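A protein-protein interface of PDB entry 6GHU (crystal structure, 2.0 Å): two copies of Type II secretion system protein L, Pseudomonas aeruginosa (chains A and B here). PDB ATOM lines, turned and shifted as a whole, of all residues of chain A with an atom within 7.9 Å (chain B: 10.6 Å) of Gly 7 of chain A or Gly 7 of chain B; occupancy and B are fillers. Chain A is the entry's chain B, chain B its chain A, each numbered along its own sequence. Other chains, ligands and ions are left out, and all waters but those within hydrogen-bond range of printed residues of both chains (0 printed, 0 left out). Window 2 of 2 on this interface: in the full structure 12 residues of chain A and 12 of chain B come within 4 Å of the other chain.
Of the printed residues of chain B, Gly 7 of chain A touches Gly 7.
Of the printed residues of chain A, Gly 7 of chain B touches Gly 7 (3.998 Å).
No residue of chain B comes within 4 Å of Gly 4 of chain A.
Of chain B, only Leu 6 comes within 4 Å of Leu 6 of chain A.
No residue of chain B comes within 4 Å of Ala 9 of chain A.
No residue of chain B comes within 4 Å of Thr 11 of chain A.
Printed residues of chain A within 4 Å of Leu 6 of chain B: Leu 6.
Printed residues of chain A within 4 Å of Leu 3 of chain B: Ala 10.
Of the printed residues of chain A, Ala 10 of chain B touches Leu 3 (3.2 Å).
Of the printed residues of chain B, Ala 10 of chain A touches Leu 3 (3.3 Å).
The nearest printed residue of chain B that does not touch Gly 7 of chain A is Ala 10 of chain B (4.2 Å).
The nearest printed residue of chain A that does not touch Gly 7 of chain B is Ala 10 of chain A (4.01 Å).
OG1 of Thr 11 of chain A is in hydrogen-bond range of O of Gly 7 of chain A.
The backbone carbonyl oxygen (O) of Gly 7 of chain B sits at hydrogen-bond distance from the side-chain hydroxyl (OG1) of Thr 11 of chain B.
Ala 10 of chain B touches Leu 3 of chain A.
Leu 6 of chain B touches Leu 6 of chain A (CD1 to CD2, 3.8 Å).
Gly 7 of chain B touches Gly 7 of chain A.
Ala 10 of chain A touches Leu 3 of chain B (CB to O, 3.3 Å).
Leu 3 of chain A touches Ala 10 of chain B, and with the chains exchanged Ala 10 of chain A touches Leu 3 of chain B.
Leu 6 of chain A touches its own counterpart, Leu 6 of chain B.
Gly 7 of chain B touches its own counterpart, Gly 7 of chain A.
Positions printed for both chains: 2, 3, 4, 5, 6, 7, 8, 9, 10, 11, 12, 13, 14 and 57.
Of the 4 pairs that touch across the chains among the printed residues, 4 have their exchanged pair printed and touching as well.
Of the 22 printed residues of chain B, 4 touch a printed residue of chain A.
Of the 14 printed residues of chain A, 4 touch a printed residue of chain B.
Printed residues of chain A that touch a printed residue of chain B: Leu 3, Leu 6, Gly 7 and Ala 10.
Hydrophobic or aromatic side chains of chain A that line the printed part of chain B: Leu 3, Leu 6 and Ala 10.
Among the printed residues, no Asp or Glu carboxylate lies within 4 Å of a Lys or Arg side-chain nitrogen of the other chain.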
ATOM      1  N   LEU A   2     -17.427   1.299 -37.448  1.00  0.00           N
ATOM      2  CA  LEU A   2     -18.728   0.966 -36.899  1.00  0.00           C
ATOM      3  C   LEU A   2     -18.717   0.744 -35.390  1.00  0.00           C
ATOM      4  O   LEU A   2     -19.759   0.386 -34.828  1.00  0.00           O
ATOM      5  CB  LEU A   2     -19.294  -0.275 -37.598  1.00  0.00           C
ATOM      6  CG  LEU A   2     -19.004  -1.635 -36.984  1.00  0.00           C
ATOM      7  CD1 LEU A   2     -19.606  -2.675 -37.900  1.00  0.00           C
ATOM      8  CD2 LEU A   2     -17.511  -1.849 -36.795  1.00  0.00           C
ATOM      9  N   LEU A   3     -17.580   0.927 -34.722  1.00  0.00           N
ATOM     10  CA  LEU A   3     -17.592   0.936 -33.265  1.00  0.00           C
ATOM     11  C   LEU A   3     -18.478   2.059 -32.747  1.00  0.00           C
ATOM     12  O   LEU A   3     -19.224   1.880 -31.777  1.00  0.00           O
ATOM     13  CB  LEU A   3     -16.169   1.074 -32.724  1.00  0.00           C
ATOM     14  N   GLY A   4     -18.417   3.228 -33.389  1.00  0.00           N
ATOM     15  CA  GLY A   4     -19.336   4.295 -33.049  1.00  0.00           C
ATOM     16  C   GLY A   4     -20.751   3.979 -33.479  1.00  0.00           C
ATOM     17  O   GLY A   4     -21.709   4.400 -32.826  1.00  0.00           O
ATOM     18  N   LEU A   5     -20.903   3.229 -34.575  1.00  0.00           N
ATOM     19  CA  LEU A   5     -22.224   2.781 -35.002  1.00  0.00           C
ATOM     20  C   LEU A   5     -22.900   1.994 -33.889  1.00  0.00           C
ATOM     21  O   LEU A   5     -24.010   2.325 -33.455  1.00  0.00           O
ATOM     22  CB  LEU A   5     -22.098   1.936 -36.272  1.00  0.00           C
ATOM     23  CG  LEU A   5     -23.355   1.399 -36.968  1.00  0.00           C
ATOM     24  CD1 LEU A   5     -23.009   0.999 -38.394  1.00  0.00           C
ATOM     25  CD2 LEU A   5     -23.968   0.204 -36.245  1.00  0.00           C
ATOM     26  N   LEU A   6     -22.230   0.949 -33.403  1.00  0.00           N
ATOM     27  CA  LEU A   6     -22.768   0.167 -32.296  1.00  0.00           C
ATOM     28  C   LEU A   6     -22.937   1.029 -31.053  1.00  0.00           C
ATOM     29  O   LEU A   6     -23.977   0.982 -30.386  1.00  0.00           O
ATOM     30  CB  LEU A   6     -21.850  -1.016 -31.997  1.00  0.00           C
ATOM     31  CG  LEU A   6     -22.396  -2.394 -32.359  1.00  0.00           C
ATOM     32  CD1 LEU A   6     -21.318  -3.450 -32.150  1.00  0.00           C
ATOM     33  CD2 LEU A   6     -23.641  -2.718 -31.535  1.00  0.00           C
ATOM     34  N   GLY A   7     -21.916   1.815 -30.722  1.00  0.00           N
ATOM     35  CA  GLY A   7     -22.009   2.682 -29.562  1.00  0.00           C
ATOM     36  C   GLY A   7     -23.159   3.664 -29.661  1.00  0.00           C
ATOM     37  O   GLY A   7     -23.882   3.887 -28.689  1.00  0.00           O
ATOM     38  N   GLN A   8     -23.347   4.262 -30.837  1.00  0.00           N
ATOM     39  CA  GLN A   8     -24.447   5.201 -31.005  1.00  0.00           C
ATOM     40  C   GLN A   8     -25.791   4.487 -30.919  1.00  0.00           C
ATOM     41  O   GLN A   8     -26.711   4.970 -30.252  1.00  0.00           O
ATOM     42  CB  GLN A   8     -24.305   5.941 -32.335  1.00  0.00           C
ATOM     43  CG  GLN A   8     -25.296   7.076 -32.506  1.00  0.00           C
ATOM     44  CD  GLN A   8     -24.907   8.013 -33.627  1.00  0.00           C
ATOM     45  OE1 GLN A   8     -23.743   8.395 -33.755  1.00  0.00           O
ATOM     46  NE2 GLN A   8     -25.878   8.390 -34.448  1.00  0.00           N
ATOM     47  N   ALA A   9     -25.916   3.325 -31.566  1.00  0.00           N
ATOM     48  CA  ALA A   9     -27.160   2.569 -31.490  1.00  0.00           C
ATOM     49  C   ALA A   9     -27.496   2.204 -30.048  1.00  0.00           C
ATOM     50  O   ALA A   9     -28.650   2.323 -29.622  1.00  0.00           O
ATOM     51  CB  ALA A   9     -27.065   1.312 -32.349  1.00  0.00           C
ATOM     52  N   ALA A  10     -26.501   1.766 -29.279  1.00  0.00           N
ATOM     53  CA  ALA A  10     -26.747   1.406 -27.887  1.00  0.00           C
ATOM     54  C   ALA A  10     -27.297   2.589 -27.098  1.00  0.00           C
ATOM     55  O   ALA A  10     -28.147   2.417 -26.218  1.00  0.00           O
ATOM     56  CB  ALA A  10     -25.460   0.894 -27.247  1.00  0.00           C
ATOM     57  N   THR A  11     -26.811   3.797 -27.388  1.00  0.00           N
ATOM     58  CA  THR A  11     -27.311   4.981 -26.699  1.00  0.00           C
ATOM     59  C   THR A  11     -28.750   5.279 -27.099  1.00  0.00           C
ATOM     60  O   THR A  11     -29.592   5.579 -26.245  1.00  0.00           O
ATOM     61  CB  THR A  11     -26.409   6.177 -27.000  1.00  0.00           C
ATOM     62  OG1 THR A  11     -25.114   5.952 -26.425  1.00  0.00           O
ATOM     63  CG2 THR A  11     -26.992   7.454 -26.427  1.00  0.00           C
ATOM     64  N   VAL A  12     -29.047   5.219 -28.396  1.00  0.00           N
ATOM     65  CA  VAL A  12     -30.403   5.492 -28.863  1.00  0.00           C
ATOM     66  C   VAL A  12     -31.368   4.444 -28.325  1.00  0.00           C
ATOM     67  O   VAL A  12     -32.448   4.770 -27.814  1.00  0.00           O
ATOM     68  CB  VAL A  12     -30.430   5.554 -30.400  1.00  0.00           C
ATOM     69  CG1 VAL A  12     -31.838   5.806 -30.915  1.00  0.00           C
ATOM     70  CG2 VAL A  12     -29.495   6.644 -30.886  1.00  0.00           C
ATOM     71  N   ILE A  13     -30.996   3.167 -28.435  1.00  0.00           N
ATOM     72  CA  ILE A  13     -31.857   2.102 -27.931  1.00  0.00           C
ATOM     73  C   ILE A  13     -32.066   2.267 -26.434  1.00  0.00           C
ATOM     74  O   ILE A  13     -33.163   2.028 -25.911  1.00  0.00           O
ATOM     75  CB  ILE A  13     -31.256   0.729 -28.283  1.00  0.00           C
ATOM     76  CG1 ILE A  13     -31.199   0.566 -29.804  1.00  0.00           C
ATOM     77  CG2 ILE A  13     -32.075  -0.398 -27.672  1.00  0.00           C
ATOM     78  CD1 ILE A  13     -30.229  -0.500 -30.286  1.00  0.00           C
ATOM     79  N   GLY A  14     -31.023   2.701 -25.726  1.00  0.00           N
ATOM     80  CA  GLY A  14     -31.126   2.951 -24.300  1.00  0.00           C
ATOM     81  C   GLY A  14     -32.135   4.021 -23.942  1.00  0.00           C
ATOM     82  O   GLY A  14     -32.646   4.024 -22.819  1.00  0.00           O
ATOM     83  N   LEU A  57     -28.069   7.112 -38.267  1.00  0.00           N
ATOM     84  CA  LEU A  57     -27.794   5.721 -38.591  1.00  0.00           C
ATOM     85  C   LEU A  57     -28.701   5.242 -39.713  1.00  0.00           C
ATOM     86  O   LEU A  57     -29.883   5.598 -39.774  1.00  0.00           O
ATOM     87  CB  LEU A  57     -27.992   4.830 -37.364  1.00  0.00           C
ATOM     88  CG  LEU A  57     -27.101   5.125 -36.160  1.00  0.00           C
ATOM     89  CD1 LEU A  57     -27.503   4.240 -34.999  1.00  0.00           C
ATOM     90  CD2 LEU A  57     -25.642   4.916 -36.515  1.00  0.00           C
ATOM     91  N   GLN B   1     -28.421  -5.178 -18.774  1.00  0.00           N
ATOM     92  CA  GLN B   1     -27.533  -4.024 -18.759  1.00  0.00           C
ATOM     93  C   GLN B   1     -26.579  -4.068 -19.954  1.00  0.00           C
ATOM     94  O   GLN B   1     -25.545  -3.400 -19.969  1.00  0.00           O
ATOM     95  CB  GLN B   1     -26.758  -3.975 -17.438  1.00  0.00           C
ATOM     96  CG  GLN B   1     -25.949  -2.701 -17.207  1.00  0.00           C
ATOM     97  CD  GLN B   1     -26.769  -1.434 -17.399  1.00  0.00           C
ATOM     98  OE1 GLN B   1     -27.997  -1.457 -17.321  1.00  0.00           O
ATOM     99  NE2 GLN B   1     -26.087  -0.321 -17.653  1.00  0.00           N
ATOM    100  N   LEU B   2     -26.908  -4.902 -20.938  1.00  0.00           N
ATOM    101  CA  LEU B   2     -26.067  -5.067 -22.121  1.00  0.00           C
ATOM    102  C   LEU B   2     -26.304  -3.975 -23.158  1.00  0.00           C
ATOM    103  O   LEU B   2     -26.295  -4.237 -24.363  1.00  0.00           O
ATOM    104  CB  LEU B   2     -26.299  -6.452 -22.722  1.00  0.00           C
ATOM    105  CG  LEU B   2     -26.116  -7.668 -21.801  1.00  0.00           C
ATOM    106  CD1 LEU B   2     -25.963  -8.938 -22.632  1.00  0.00           C
ATOM    107  CD2 LEU B   2     -24.932  -7.515 -20.856  1.00  0.00           C
ATOM    108  N   LEU B   3     -26.534  -2.745 -22.702  1.00  0.00           N
ATOM    109  CA  LEU B   3     -26.634  -1.575 -23.564  1.00  0.00           C
ATOM    110  C   LEU B   3     -25.573  -0.540 -23.231  1.00  0.00           C
ATOM    111  O   LEU B   3     -24.918  -0.015 -24.138  1.00  0.00           O
ATOM    112  CB  LEU B   3     -28.035  -0.948 -23.451  1.00  0.00           C
ATOM    113  N   GLY B   4     -25.383  -0.227 -21.947  1.00  0.00           N
ATOM    114  CA  GLY B   4     -24.223   0.551 -21.562  1.00  0.00           C
ATOM    115  C   GLY B   4     -22.943  -0.223 -21.776  1.00  0.00           C
ATOM    116  O   GLY B   4     -21.911   0.356 -22.122  1.00  0.00           O
ATOM    117  N   LEU B   5     -23.001  -1.545 -21.599  1.00  0.00           N
ATOM    118  CA  LEU B   5     -21.827  -2.385 -21.790  1.00  0.00           C
ATOM    119  C   LEU B   5     -21.341  -2.316 -23.232  1.00  0.00           C
ATOM    120  O   LEU B   5     -20.149  -2.114 -23.492  1.00  0.00           O
ATOM    121  CB  LEU B   5     -22.165  -3.820 -21.392  1.00  0.00           C
ATOM    122  CG  LEU B   5     -21.052  -4.863 -21.445  1.00  0.00           C
ATOM    123  CD1 LEU B   5     -21.372  -5.971 -20.458  1.00  0.00           C
ATOM    124  CD2 LEU B   5     -20.885  -5.436 -22.852  1.00  0.00           C
ATOM    125  N   LEU B   6     -22.256  -2.495 -24.184  1.00  0.00           N
ATOM    126  CA  LEU B   6     -21.913  -2.354 -25.594  1.00  0.00           C
ATOM    127  C   LEU B   6     -21.236  -1.021 -25.866  1.00  0.00           C
ATOM    128  O   LEU B   6     -20.118  -0.963 -26.391  1.00  0.00           O
ATOM    129  CB  LEU B   6     -23.171  -2.463 -26.448  1.00  0.00           C
ATOM    130  CG  LEU B   6     -23.611  -3.809 -26.999  1.00  0.00           C
ATOM    131  CD1 LEU B   6     -24.735  -3.512 -27.984  1.00  0.00           C
ATOM    132  CD2 LEU B   6     -22.464  -4.578 -27.656  1.00  0.00           C
ATOM    133  N   GLY B   7     -21.930   0.069 -25.544  1.00  0.00           N
ATOM    134  CA  GLY B   7     -21.396   1.386 -25.830  1.00  0.00           C
ATOM    135  C   GLY B   7     -20.048   1.615 -25.181  1.00  0.00           C
ATOM    136  O   GLY B   7     -19.149   2.203 -25.788  1.00  0.00           O
ATOM    137  N   GLN B   8     -19.884   1.155 -23.942  1.00  0.00           N
ATOM    138  CA  GLN B   8     -18.620   1.374 -23.253  1.00  0.00           C
ATOM    139  C   GLN B   8     -17.505   0.560 -23.900  1.00  0.00           C
ATOM    140  O   GLN B   8     -16.415   1.082 -24.153  1.00  0.00           O
ATOM    141  CB  GLN B   8     -18.757   1.039 -21.767  1.00  0.00           C
ATOM    142  CG  GLN B   8     -17.507   1.401 -20.971  1.00  0.00           C
ATOM    143  CD  GLN B   8     -17.763   1.569 -19.489  1.00  0.00           C
ATOM    144  OE1 GLN B   8     -17.073   0.975 -18.660  1.00  0.00           O
ATOM    145  NE2 GLN B   8     -18.737   2.402 -19.145  1.00  0.00           N
ATOM    146  N   ALA B   9     -17.768  -0.717 -24.193  1.00  0.00           N
ATOM    147  CA  ALA B   9     -16.766  -1.541 -24.858  1.00  0.00           C
ATOM    148  C   ALA B   9     -16.373  -0.949 -26.205  1.00  0.00           C
ATOM    149  O   ALA B   9     -15.188  -0.896 -26.543  1.00  0.00           O
ATOM    150  CB  ALA B   9     -17.286  -2.967 -25.031  1.00  0.00           C
ATOM    151  N   ALA B  10     -17.353  -0.490 -26.985  1.00  0.00           N
ATOM    152  CA  ALA B  10     -17.055   0.073 -28.299  1.00  0.00           C
ATOM    153  C   ALA B  10     -16.148   1.294 -28.187  1.00  0.00           C
ATOM    154  O   ALA B  10     -15.252   1.489 -29.015  1.00  0.00           O
ATOM    155  CB  ALA B  10     -18.353   0.439 -29.019  1.00  0.00           C
ATOM    156  N   THR B  11     -16.376   2.133 -27.177  1.00  0.00           N
ATOM    157  CA  THR B  11     -15.520   3.294 -26.964  1.00  0.00           C
ATOM    158  C   THR B  11     -14.109   2.872 -26.578  1.00  0.00           C
ATOM    159  O   THR B  11     -13.127   3.459 -27.044  1.00  0.00           O
ATOM    160  CB  THR B  11     -16.121   4.188 -25.880  1.00  0.00           C
ATOM    161  OG1 THR B  11     -17.407   4.654 -26.305  1.00  0.00           O
ATOM    162  CG2 THR B  11     -15.225   5.376 -25.606  1.00  0.00           C
ATOM    163  N   VAL B  12     -13.990   1.872 -25.706  1.00  0.00           N
ATOM    164  CA  VAL B  12     -12.676   1.413 -25.270  1.00  0.00           C
ATOM    165  C   VAL B  12     -11.928   0.761 -26.424  1.00  0.00           C
ATOM    166  O   VAL B  12     -10.737   1.013 -26.630  1.00  0.00           O
ATOM    167  CB  VAL B  12     -12.822   0.452 -24.079  1.00  0.00           C
ATOM    168  CG1 VAL B  12     -11.476  -0.158 -23.713  1.00  0.00           C
ATOM    169  CG2 VAL B  12     -13.413   1.189 -22.897  1.00  0.00           C
ATOM    170  N   ILE B  13     -12.608  -0.101 -27.185  1.00  0.00           N
ATOM    171  CA  ILE B  13     -11.947  -0.761 -28.307  1.00  0.00           C
ATOM    172  C   ILE B  13     -11.539   0.263 -29.355  1.00  0.00           C
ATOM    173  O   ILE B  13     -10.522   0.094 -30.041  1.00  0.00           O
ATOM    174  CB  ILE B  13     -12.859  -1.857 -28.890  1.00  0.00           C
ATOM    175  CG1 ILE B  13     -13.134  -2.915 -27.824  1.00  0.00           C
ATOM    176  CG2 ILE B  13     -12.210  -2.522 -30.097  1.00  0.00           C
ATOM    177  CD1 ILE B  13     -14.346  -3.768 -28.095  1.00  0.00           C
ATOM    178  N   GLY B  14     -12.305   1.347 -29.484  1.00  0.00           N
ATOM    179  CA  GLY B  14     -11.933   2.420 -30.388  1.00  0.00           C
ATOM    180  C   GLY B  14     -10.668   3.143 -29.985  1.00  0.00           C
ATOM    181  O   GLY B  14     -10.019   3.757 -30.835  1.00  0.00           O
ATOM    182  N   GLY B  15     -10.313   3.097 -28.703  1.00  0.00           N
ATOM    183  CA  GLY B  15      -9.041   3.615 -28.249  1.00  0.00           C
ATOM    184  C   GLY B  15      -7.857   2.744 -28.590  1.00  0.00           C
ATOM    185  O   GLY B  15      -6.725   3.085 -28.229  1.00  0.00           O
ATOM    186  N   LEU B  24     -19.045 -10.092 -33.709  1.00  0.00           N
ATOM    187  CA  LEU B  24     -19.495  -9.809 -32.356  1.00  0.00           C
ATOM    188  C   LEU B  24     -20.912 -10.332 -32.220  1.00  0.00           C
ATOM    189  O   LEU B  24     -21.698 -10.251 -33.168  1.00  0.00           O
ATOM    190  CB  LEU B  24     -19.425  -8.309 -32.045  1.00  0.00           C
ATOM    191  CG  LEU B  24     -20.105  -7.807 -30.763  1.00  0.00           C
ATOM    192  CD1 LEU B  24     -19.405  -6.562 -30.249  1.00  0.00           C
ATOM    193  CD2 LEU B  24     -21.584  -7.493 -30.983  1.00  0.00           C
ATOM    194  N   VAL B  33     -21.353 -10.760 -23.982  1.00  0.00           N
ATOM    195  CA  VAL B  33     -21.006 -10.317 -25.326  1.00  0.00           C
ATOM    196  C   VAL B  33     -19.698 -10.985 -25.727  1.00  0.00           C
ATOM    197  O   VAL B  33     -18.699 -10.889 -25.003  1.00  0.00           O
ATOM    198  CB  VAL B  33     -20.875  -8.785 -25.393  1.00  0.00           C
ATOM    199  CG1 VAL B  33     -20.660  -8.330 -26.829  1.00  0.00           C
ATOM    200  CG2 VAL B  33     -22.097  -8.108 -24.785  1.00  0.00           C
ATOM    201  N   LEU B  35     -16.723 -11.302 -28.715  1.00  0.00           N
ATOM    202  CA  LEU B  35     -16.100 -10.600 -29.830  1.00  0.00           C
ATOM    203  C   LEU B  35     -14.940 -11.425 -30.363  1.00  0.00           C
ATOM    204  O   LEU B  35     -14.117 -11.916 -29.585  1.00  0.00           O
ATOM    205  CB  LEU B  35     -15.573  -9.217 -29.417  1.00  0.00           C
ATOM    206  CG  LEU B  35     -16.481  -8.235 -28.679  1.00  0.00           C
ATOM    207  CD1 LEU B  35     -16.576  -8.570 -27.198  1.00  0.00           C
ATOM    208  CD2 LEU B  35     -15.957  -6.812 -28.874  1.00  0.00           C
ATOM    209  N   LEU B  52     -10.454  -2.440 -21.005  1.00  0.00           N
ATOM    210  CA  LEU B  52     -11.847  -2.798 -20.767  1.00  0.00           C
ATOM    211  C   LEU B  52     -12.098  -3.015 -19.281  1.00  0.00           C
ATOM    212  O   LEU B  52     -13.068  -2.495 -18.716  1.00  0.00           O
ATOM    213  CB  LEU B  52     -12.208  -4.050 -21.567  1.00  0.00           C
ATOM    214  CG  LEU B  52     -12.271  -3.859 -23.083  1.00  0.00           C
ATOM    215  CD1 LEU B  52     -12.255  -5.204 -23.785  1.00  0.00           C
ATOM    216  CD2 LEU B  52     -13.511  -3.058 -23.470  1.00  0.00           C
ATOM    217  N   SER B  55     -12.088   0.167 -17.277  1.00  0.00           N
ATOM    218  CA  SER B  55     -13.323   0.923 -17.445  1.00  0.00           C
ATOM    219  C   SER B  55     -14.462   0.362 -16.612  1.00  0.00           C
ATOM    220  O   SER B  55     -15.546   0.955 -16.595  1.00  0.00           O
ATOM    221  CB  SER B  55     -13.739   0.949 -18.915  1.00  0.00           C
ATOM    222  OG  SER B  55     -14.347  -0.273 -19.301  1.00  0.00           O
ATOM    223  N   LEU B  57     -15.576  -3.030 -16.816  1.00  0.00           N
ATOM    224  CA  LEU B  57     -16.250  -4.151 -17.451  1.00  0.00           C
ATOM    225  C   LEU B  57     -15.615  -5.468 -17.038  1.00  0.00           C
ATOM    226  O   LEU B  57     -14.389  -5.578 -16.937  1.00  0.00           O
ATOM    227  CB  LEU B  57     -16.201  -4.020 -18.973  1.00  0.00           C
ATOM    228  CG  LEU B  57     -16.788  -2.732 -19.549  1.00  0.00           C
ATOM    229  CD1 LEU B  57     -16.492  -2.643 -21.037  1.00  0.00           C
ATOM    230  CD2 LEU B  57     -18.288  -2.653 -19.290  1.00  0.00           C
ATOM    231  N   ILE B  77     -17.180 -10.145 -22.879  1.00  0.00           N
ATOM    232  CA  ILE B  77     -17.460  -9.047 -21.962  1.00  0.00           C
ATOM    233  C   ILE B  77     -18.783  -9.335 -21.266  1.00  0.00           C
ATOM    234  O   ILE B  77     -19.806  -9.558 -21.927  1.00  0.00           O
ATOM    235  CB  ILE B  77     -17.495  -7.694 -22.690  1.00  0.00           C
ATOM    236  CG1 ILE B  77     -16.159  -7.441 -23.395  1.00  0.00           C
ATOM    237  CG2 ILE B  77     -17.767  -6.572 -21.703  1.00  0.00           C
ATOM    238  CD1 ILE B  77     -16.164  -6.245 -24.335  1.00  0.00           C
